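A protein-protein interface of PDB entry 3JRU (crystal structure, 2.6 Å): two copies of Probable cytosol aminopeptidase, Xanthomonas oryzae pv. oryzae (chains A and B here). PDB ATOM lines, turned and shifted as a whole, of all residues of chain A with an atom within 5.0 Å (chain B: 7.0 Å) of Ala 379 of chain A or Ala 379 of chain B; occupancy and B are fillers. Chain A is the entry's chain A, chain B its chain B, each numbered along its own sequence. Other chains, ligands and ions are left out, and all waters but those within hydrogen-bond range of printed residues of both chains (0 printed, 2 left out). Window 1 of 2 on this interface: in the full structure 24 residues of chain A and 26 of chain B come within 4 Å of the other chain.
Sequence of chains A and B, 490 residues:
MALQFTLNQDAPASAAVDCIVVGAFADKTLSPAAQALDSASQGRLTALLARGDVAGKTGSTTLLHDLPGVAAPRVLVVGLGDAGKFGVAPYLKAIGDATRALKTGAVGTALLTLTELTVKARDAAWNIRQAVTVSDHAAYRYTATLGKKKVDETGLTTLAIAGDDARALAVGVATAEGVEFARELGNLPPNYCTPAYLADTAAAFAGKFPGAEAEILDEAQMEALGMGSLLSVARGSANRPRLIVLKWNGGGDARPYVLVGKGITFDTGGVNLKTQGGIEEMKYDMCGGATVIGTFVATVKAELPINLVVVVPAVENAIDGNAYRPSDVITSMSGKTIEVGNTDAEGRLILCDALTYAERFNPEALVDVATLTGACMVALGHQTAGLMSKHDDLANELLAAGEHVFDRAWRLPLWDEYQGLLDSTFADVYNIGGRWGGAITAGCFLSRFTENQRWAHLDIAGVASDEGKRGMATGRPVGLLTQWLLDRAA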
ATOM      1  N   ALA A 375       0.134  22.529 -12.159  1.00  0.00           N
ATOM      2  CA  ALA A 375      -0.284  21.407 -11.313  1.00  0.00           C
ATOM      3  C   ALA A 375      -0.271  21.766  -9.818  1.00  0.00           C
ATOM      4  O   ALA A 375      -1.230  21.451  -9.096  1.00  0.00           O
ATOM      5  CB  ALA A 375       0.551  20.166 -11.590  1.00  0.00           C
ATOM      6  N   CYS A 376       0.789  22.441  -9.356  1.00  0.00           N
ATOM      7  CA  CYS A 376       0.899  22.823  -7.930  1.00  0.00           C
ATOM      8  C   CYS A 376      -0.152  23.816  -7.460  1.00  0.00           C
ATOM      9  O   CYS A 376      -0.603  23.747  -6.314  1.00  0.00           O
ATOM     10  CB  CYS A 376       2.258  23.427  -7.659  1.00  0.00           C
ATOM     11  SG  CYS A 376       2.621  23.629  -5.940  1.00  0.00           S
ATOM     12  N   MET A 377      -0.510  24.749  -8.340  1.00  0.00           N
ATOM     13  CA  MET A 377      -1.686  25.598  -8.128  1.00  0.00           C
ATOM     14  C   MET A 377      -3.021  24.828  -7.990  1.00  0.00           C
ATOM     15  O   MET A 377      -3.822  25.045  -7.057  1.00  0.00           O
ATOM     16  CB  MET A 377      -1.771  26.643  -9.223  1.00  0.00           C
ATOM     17  CG  MET A 377      -0.628  27.634  -9.134  1.00  0.00           C
ATOM     18  SD  MET A 377      -0.905  29.126 -10.086  1.00  0.00           S
ATOM     19  CE  MET A 377      -0.029  28.737 -11.623  1.00  0.00           C
ATOM     20  N   VAL A 378      -3.255  23.910  -8.913  1.00  0.00           N
ATOM     21  CA  VAL A 378      -4.416  23.043  -8.800  1.00  0.00           C
ATOM     22  C   VAL A 378      -4.342  22.307  -7.428  1.00  0.00           C
ATOM     23  O   VAL A 378      -5.302  22.299  -6.665  1.00  0.00           O
ATOM     24  CB  VAL A 378      -4.552  22.084 -10.044  1.00  0.00           C
ATOM     25  CG1 VAL A 378      -5.698  21.143  -9.844  1.00  0.00           C
ATOM     26  CG2 VAL A 378      -4.719  22.866 -11.408  1.00  0.00           C
ATOM     27  N   ALA A 379      -3.170  21.754  -7.099  1.00  0.00           N
ATOM     28  CA  ALA A 379      -2.947  21.033  -5.827  1.00  0.00           C
ATOM     29  C   ALA A 379      -3.157  21.873  -4.575  1.00  0.00           C
ATOM     30  O   ALA A 379      -3.893  21.464  -3.679  1.00  0.00           O
ATOM     31  CB  ALA A 379      -1.559  20.451  -5.794  1.00  0.00           C
ATOM     32  N   LEU A 380      -2.511  23.046  -4.517  1.00  0.00           N
ATOM     33  CA  LEU A 380      -2.374  23.780  -3.250  1.00  0.00           C
ATOM     34  C   LEU A 380      -2.952  25.205  -3.199  1.00  0.00           C
ATOM     35  O   LEU A 380      -3.084  25.775  -2.107  1.00  0.00           O
ATOM     36  CB  LEU A 380      -0.921  23.699  -2.733  1.00  0.00           C
ATOM     37  CG  LEU A 380      -0.588  22.290  -2.220  1.00  0.00           C
ATOM     38  CD1 LEU A 380       0.918  22.047  -2.112  1.00  0.00           C
ATOM     39  CD2 LEU A 380      -1.328  22.007  -0.875  1.00  0.00           C
ATOM     40  N   GLY A 381      -3.319  25.764  -4.354  1.00  0.00           N
ATOM     41  CA  GLY A 381      -3.956  27.089  -4.424  1.00  0.00           C
ATOM     42  C   GLY A 381      -2.977  28.258  -4.446  1.00  0.00           C
ATOM     43  O   GLY A 381      -1.762  28.081  -4.652  1.00  0.00           O
ATOM     44  N   LEU A 412       4.509  17.317  -0.715  1.00  0.00           N
ATOM     45  CA  LEU A 412       3.960  16.413  -1.702  1.00  0.00           C
ATOM     46  C   LEU A 412       4.986  15.313  -1.846  1.00  0.00           C
ATOM     47  O   LEU A 412       6.180  15.564  -1.751  1.00  0.00           O
ATOM     48  CB  LEU A 412       3.774  17.121  -3.033  1.00  0.00           C
ATOM     49  CG  LEU A 412       2.708  18.218  -3.086  1.00  0.00           C
ATOM     50  CD1 LEU A 412       2.616  18.726  -4.456  1.00  0.00           C
ATOM     51  CD2 LEU A 412       1.302  17.771  -2.616  1.00  0.00           C
ATOM     52  N   GLY A 437      -0.304  14.375 -11.669  1.00  0.00           N
ATOM     53  CA  GLY A 437       0.872  14.376 -10.806  1.00  0.00           C
ATOM     54  C   GLY A 437       1.907  15.384 -11.258  1.00  0.00           C
ATOM     55  O   GLY A 437       3.077  15.223 -10.938  1.00  0.00           O
ATOM     56  N   ILE A 440       4.501  16.791  -8.901  1.00  0.00           N
ATOM     57  CA  ILE A 440       5.327  15.692  -8.378  1.00  0.00           C
ATOM     58  C   ILE A 440       6.370  15.245  -9.387  1.00  0.00           C
ATOM     59  O   ILE A 440       7.547  15.078  -9.058  1.00  0.00           O
ATOM     60  CB  ILE A 440       4.461  14.462  -7.928  1.00  0.00           C
ATOM     61  CG1 ILE A 440       3.632  14.821  -6.696  1.00  0.00           C
ATOM     62  CG2 ILE A 440       5.338  13.271  -7.571  1.00  0.00           C
ATOM     63  CD1 ILE A 440       2.572  13.810  -6.371  1.00  0.00           C
ATOM     64  N   GLY B 374     -10.966  15.927 -10.479  1.00  0.00           N
ATOM     65  CA  GLY B 374      -9.811  16.037 -11.353  1.00  0.00           C
ATOM     66  C   GLY B 374      -8.633  16.694 -10.627  1.00  0.00           C
ATOM     67  O   GLY B 374      -7.490  16.244 -10.793  1.00  0.00           O
ATOM     68  N   ALA B 375      -8.897  17.743  -9.818  1.00  0.00           N
ATOM     69  CA  ALA B 375      -7.832  18.439  -9.039  1.00  0.00           C
ATOM     70  C   ALA B 375      -6.910  17.481  -8.267  1.00  0.00           C
ATOM     71  O   ALA B 375      -5.694  17.558  -8.345  1.00  0.00           O
ATOM     72  CB  ALA B 375      -8.419  19.448  -8.108  1.00  0.00           C
ATOM     73  N   CYS B 376      -7.510  16.549  -7.553  1.00  0.00           N
ATOM     74  CA  CYS B 376      -6.752  15.550  -6.808  1.00  0.00           C
ATOM     75  C   CYS B 376      -5.908  14.712  -7.761  1.00  0.00           C
ATOM     76  O   CYS B 376      -4.765  14.390  -7.437  1.00  0.00           O
ATOM     77  CB  CYS B 376      -7.702  14.665  -5.984  1.00  0.00           C
ATOM     78  SG  CYS B 376      -6.879  13.629  -4.731  1.00  0.00           S
ATOM     79  N   MET B 377      -6.457  14.366  -8.927  1.00  0.00           N
ATOM     80  CA  MET B 377      -5.694  13.639  -9.914  1.00  0.00           C
ATOM     81  C   MET B 377      -4.505  14.483 -10.395  1.00  0.00           C
ATOM     82  O   MET B 377      -3.399  13.976 -10.568  1.00  0.00           O
ATOM     83  CB  MET B 377      -6.568  13.232 -11.092  1.00  0.00           C
ATOM     84  CG  MET B 377      -7.666  12.202 -10.791  1.00  0.00           C
ATOM     85  SD  MET B 377      -8.177  11.410 -12.341  1.00  0.00           S
ATOM     86  CE  MET B 377      -9.543  12.485 -12.777  1.00  0.00           C
ATOM     87  N   VAL B 378      -4.722  15.769 -10.589  1.00  0.00           N
ATOM     88  CA  VAL B 378      -3.630  16.661 -10.936  1.00  0.00           C
ATOM     89  C   VAL B 378      -2.621  16.695  -9.801  1.00  0.00           C
ATOM     90  O   VAL B 378      -1.404  16.699 -10.041  1.00  0.00           O
ATOM     91  CB  VAL B 378      -4.109  18.102 -11.323  1.00  0.00           C
ATOM     92  CG1 VAL B 378      -2.924  19.025 -11.552  1.00  0.00           C
ATOM     93  CG2 VAL B 378      -5.015  18.059 -12.575  1.00  0.00           C
ATOM     94  N   ALA B 379      -3.121  16.665  -8.568  1.00  0.00           N
ATOM     95  CA  ALA B 379      -2.245  16.757  -7.395  1.00  0.00           C
ATOM     96  C   ALA B 379      -1.407  15.501  -7.177  1.00  0.00           C
ATOM     97  O   ALA B 379      -0.187  15.596  -6.888  1.00  0.00           O
ATOM     98  CB  ALA B 379      -3.037  17.126  -6.116  1.00  0.00           C
ATOM     99  N   LEU B 380      -2.033  14.328  -7.329  1.00  0.00           N
ATOM    100  CA  LEU B 380      -1.423  13.089  -6.820  1.00  0.00           C
ATOM    101  C   LEU B 380      -1.395  11.934  -7.820  1.00  0.00           C
ATOM    102  O   LEU B 380      -0.801  10.880  -7.543  1.00  0.00           O
ATOM    103  CB  LEU B 380      -2.120  12.681  -5.543  1.00  0.00           C
ATOM    104  CG  LEU B 380      -1.963  13.679  -4.370  1.00  0.00           C
ATOM    105  CD1 LEU B 380      -3.042  13.494  -3.204  1.00  0.00           C
ATOM    106  CD2 LEU B 380      -0.510  13.654  -3.824  1.00  0.00           C
ATOM    107  N   GLY B 381      -2.020  12.132  -8.982  1.00  0.00           N
ATOM    108  CA  GLY B 381      -1.976  11.134 -10.024  1.00  0.00           C
ATOM    109  C   GLY B 381      -2.883   9.943  -9.737  1.00  0.00           C
ATOM    110  O   GLY B 381      -3.790  10.006  -8.856  1.00  0.00           O
ATOM    111  N   THR B 384      -1.852   7.762  -5.769  1.00  0.00           N
ATOM    112  CA  THR B 384      -2.135   7.983  -4.355  1.00  0.00           C
ATOM    113  C   THR B 384      -3.412   8.750  -4.152  1.00  0.00           C
ATOM    114  O   THR B 384      -3.653   9.721  -4.861  1.00  0.00           O
ATOM    115  CB  THR B 384      -1.034   8.879  -3.753  1.00  0.00           C
ATOM    116  OG1 THR B 384       0.251   8.453  -4.241  1.00  0.00           O
ATOM    117  CG2 THR B 384      -1.096   8.889  -2.233  1.00  0.00           C
ATOM    118  N   LEU B 412      -3.818  16.154   2.462  1.00  0.00           N
ATOM    119  CA  LEU B 412      -3.847  17.548   2.013  1.00  0.00           C
ATOM    120  C   LEU B 412      -4.511  18.375   3.107  1.00  0.00           C
ATOM    121  O   LEU B 412      -5.310  17.842   3.878  1.00  0.00           O
ATOM    122  CB  LEU B 412      -4.647  17.699   0.727  1.00  0.00           C
ATOM    123  CG  LEU B 412      -4.089  16.932  -0.445  1.00  0.00           C
ATOM    124  CD1 LEU B 412      -5.101  17.002  -1.562  1.00  0.00           C
ATOM    125  CD2 LEU B 412      -2.675  17.425  -0.873  1.00  0.00           C
ATOM    126  N   PRO B 413      -4.195  19.679   3.176  1.00  0.00           N
ATOM    127  CA  PRO B 413      -4.674  20.411   4.342  1.00  0.00           C
ATOM    128  C   PRO B 413      -6.116  20.949   4.170  1.00  0.00           C
ATOM    129  O   PRO B 413      -6.559  21.205   3.040  1.00  0.00           O
ATOM    130  CB  PRO B 413      -3.679  21.574   4.424  1.00  0.00           C
ATOM    131  CG  PRO B 413      -3.308  21.874   2.938  1.00  0.00           C
ATOM    132  CD  PRO B 413      -3.308  20.494   2.303  1.00  0.00           C
ATOM    133  N   TYR B 418      -8.575  28.446   3.190  1.00  0.00           N
ATOM    134  CA  TYR B 418      -9.204  27.886   1.990  1.00  0.00           C
ATOM    135  C   TYR B 418     -10.704  28.123   1.995  1.00  0.00           C
ATOM    136  O   TYR B 418     -11.314  28.157   0.949  1.00  0.00           O
ATOM    137  CB  TYR B 418      -8.901  26.386   1.832  1.00  0.00           C
ATOM    138  CG  TYR B 418      -7.469  26.106   1.467  1.00  0.00           C
ATOM    139  CD1 TYR B 418      -6.998  26.430   0.210  1.00  0.00           C
ATOM    140  CD2 TYR B 418      -6.578  25.531   2.389  1.00  0.00           C
ATOM    141  CE1 TYR B 418      -5.700  26.203  -0.154  1.00  0.00           C
ATOM    142  CE2 TYR B 418      -5.250  25.272   2.041  1.00  0.00           C
ATOM    143  CZ  TYR B 418      -4.814  25.617   0.755  1.00  0.00           C
ATOM    144  OH  TYR B 418      -3.500  25.428   0.345  1.00  0.00           O
ATOM    145  N   TRP B 436      -8.331  27.008  -8.624  1.00  0.00           N
ATOM    146  CA  TRP B 436      -7.196  26.492  -7.815  1.00  0.00           C
ATOM    147  C   TRP B 436      -7.550  25.877  -6.464  1.00  0.00           C
ATOM    148  O   TRP B 436      -8.383  26.413  -5.725  1.00  0.00           O
ATOM    149  CB  TRP B 436      -6.130  27.579  -7.576  1.00  0.00           C
ATOM    150  CG  TRP B 436      -5.885  28.440  -8.752  1.00  0.00           C
ATOM    151  CD1 TRP B 436      -6.068  29.783  -8.832  1.00  0.00           C
ATOM    152  CD2 TRP B 436      -5.418  28.012 -10.041  1.00  0.00           C
ATOM    153  NE1 TRP B 436      -5.727  30.230 -10.087  1.00  0.00           N
ATOM    154  CE2 TRP B 436      -5.328  29.164 -10.851  1.00  0.00           C
ATOM    155  CE3 TRP B 436      -5.066  26.757 -10.586  1.00  0.00           C
ATOM    156  CZ2 TRP B 436      -4.894  29.118 -12.188  1.00  0.00           C
ATOM    157  CZ3 TRP B 436      -4.641  26.703 -11.909  1.00  0.00           C
ATOM    158  CH2 TRP B 436      -4.553  27.892 -12.704  1.00  0.00           C
ATOM    159  N   GLY B 437      -6.872  24.768  -6.156  1.00  0.00           N
ATOM    160  CA  GLY B 437      -7.009  24.091  -4.875  1.00  0.00           C
ATOM    161  C   GLY B 437      -8.276  23.269  -4.741  1.00  0.00           C
ATOM    162  O   GLY B 437      -8.760  23.074  -3.624  1.00  0.00           O
ATOM    163  N   GLY B 438      -8.780  22.768  -5.872  1.00  0.00           N
ATOM    164  CA  GLY B 438     -10.098  22.116  -5.958  1.00  0.00           C
ATOM    165  C   GLY B 438     -10.314  20.865  -5.138  1.00  0.00           C
ATOM    166  O   GLY B 438     -11.458  20.537  -4.805  1.00  0.00           O
ATOM    167  N   ALA B 439      -9.232  20.159  -4.801  1.00  0.00           N
ATOM    168  CA  ALA B 439      -9.352  18.916  -4.040  1.00  0.00           C
ATOM    169  C   ALA B 439      -9.607  19.304  -2.616  1.00  0.00           C
ATOM    170  O   ALA B 439     -10.451  18.728  -1.947  1.00  0.00           O
ATOM    171  CB  ALA B 439      -8.092  18.067  -4.144  1.00  0.00           C
ATOM    172  N   ILE B 440      -8.859  20.304  -2.183  1.00  0.00           N
ATOM    173  CA  ILE B 440      -8.927  20.840  -0.872  1.00  0.00           C
ATOM    174  C   ILE B 440     -10.271  21.539  -0.698  1.00  0.00           C
ATOM    175  O   ILE B 440     -10.933  21.350   0.304  1.00  0.00           O
ATOM    176  CB  ILE B 440      -7.796  21.851  -0.701  1.00  0.00           C
ATOM    177  CG1 ILE B 440      -6.467  21.114  -0.687  1.00  0.00           C
ATOM    178  CG2 ILE B 440      -7.998  22.731   0.518  1.00  0.00           C
ATOM    179  CD1 ILE B 440      -5.301  22.040  -0.711  1.00  0.00           C
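The backbone NH of Gly 437 of chain A is in hydrogen-bond range of the backbone carbonyl oxygen of Val 378 of chain B (3.0 Å).
The backbone NH (N) of Gly 437 of chain B lies within hydrogen-bond range of the backbone carbonyl oxygen (O) of Val 378 of chain A (3.0 Å).
N of Gly 437 of chain B is in hydrogen-bond range of O of Met 377 of chain A (3.2 Å).
OH of Tyr 418 of chain B sits at hydrogen-bond distance from O of Leu 380 of chain A.
O of Met 377 of chain B is in hydrogen-bond range of N of Gly 437 of chain A (3.3 Å).
Of chain B, only Ala 379 and Ile 440 come within 4 Å of Ala 379 of chain A.
Of the printed residues of chain B, Gly 437 of chain A touches Met 377, Val 378 and Gly 381.
Printed residues of chain B within 4 Å of Ala 375 of chain A: Val 378.
Printed residues of chain B within 4 Å of Ile 440 of chain A: Ala 379 (3.3 Å).
The nearest residue of chain B that does not touch Ala 379 of chain A is Gly 437 of chain B (4.2 Å).
The nearest residue of chain A that does not touch Ala 379 of chain B is Gly 437 of chain A (4.2 Å).
Val 378 of chain A touches Gly 437 of chain B, and with the chains exchanged Gly 437 of chain A touches Val 378 of chain B.
Ala 379 of chain A touches its own counterpart, Ala 379 of chain B.
Ala 379 of chain A touches Ile 440 of chain B, and with the chains exchanged Ile 440 of chain A touches Ala 379 of chain B.
Gly 437 of chain A touches Gly 381 of chain B, but with the chains exchanged Gly 381 of chain A does not touch Gly 437 of chain B (4.1 Å).
10 positions are printed for both chains.
Ala 375 of chain A touches Val 378 of chain B (CA to CG1, 3.6 Å).
CB of Trp 436 of chain B touches O of Met 377 of chain A, at 3.5 Å.
CA of Ala 375 of chain B touches CG1 of Val 378 of chain A (3.5 Å).
Val 378 of chain A touches Gly 438 of chain B.
CB of Ala 379 of chain A touches CB of Ala 379 of chain B (3.7 Å).
Ile 440 of chain B touches Ala 379 of chain A.
CD2 of Leu 380 of chain A touches CD1 of Ile 440 of chain B, at 3.98 Å.
Gly 381 of chain A touches Trp 436 of chain B (CA to CB, 3.9 Å).
N of Gly 437 of chain A touches N of Gly 381 of chain B, at 3.9 Å.
O of Ala 379 of chain B touches CD1 of Ile 440 of chain A (3.3 Å).
Of the 17 printed residues of chain B, 10 touch a printed residue of chain A.
Hydrophobic or aromatic side chains of chain B that line the printed part of chain A: Ala 375, Val 378, Ala 379, Tyr 418, Trp 436 and Ile 440.
Of the 10 printed residues of chain A, 8 touch a printed residue of chain B.
Among the printed residues, no Asp or Glu carboxylate lies within 4 Å of a Lys or Arg side-chain nitrogen of the other chain.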
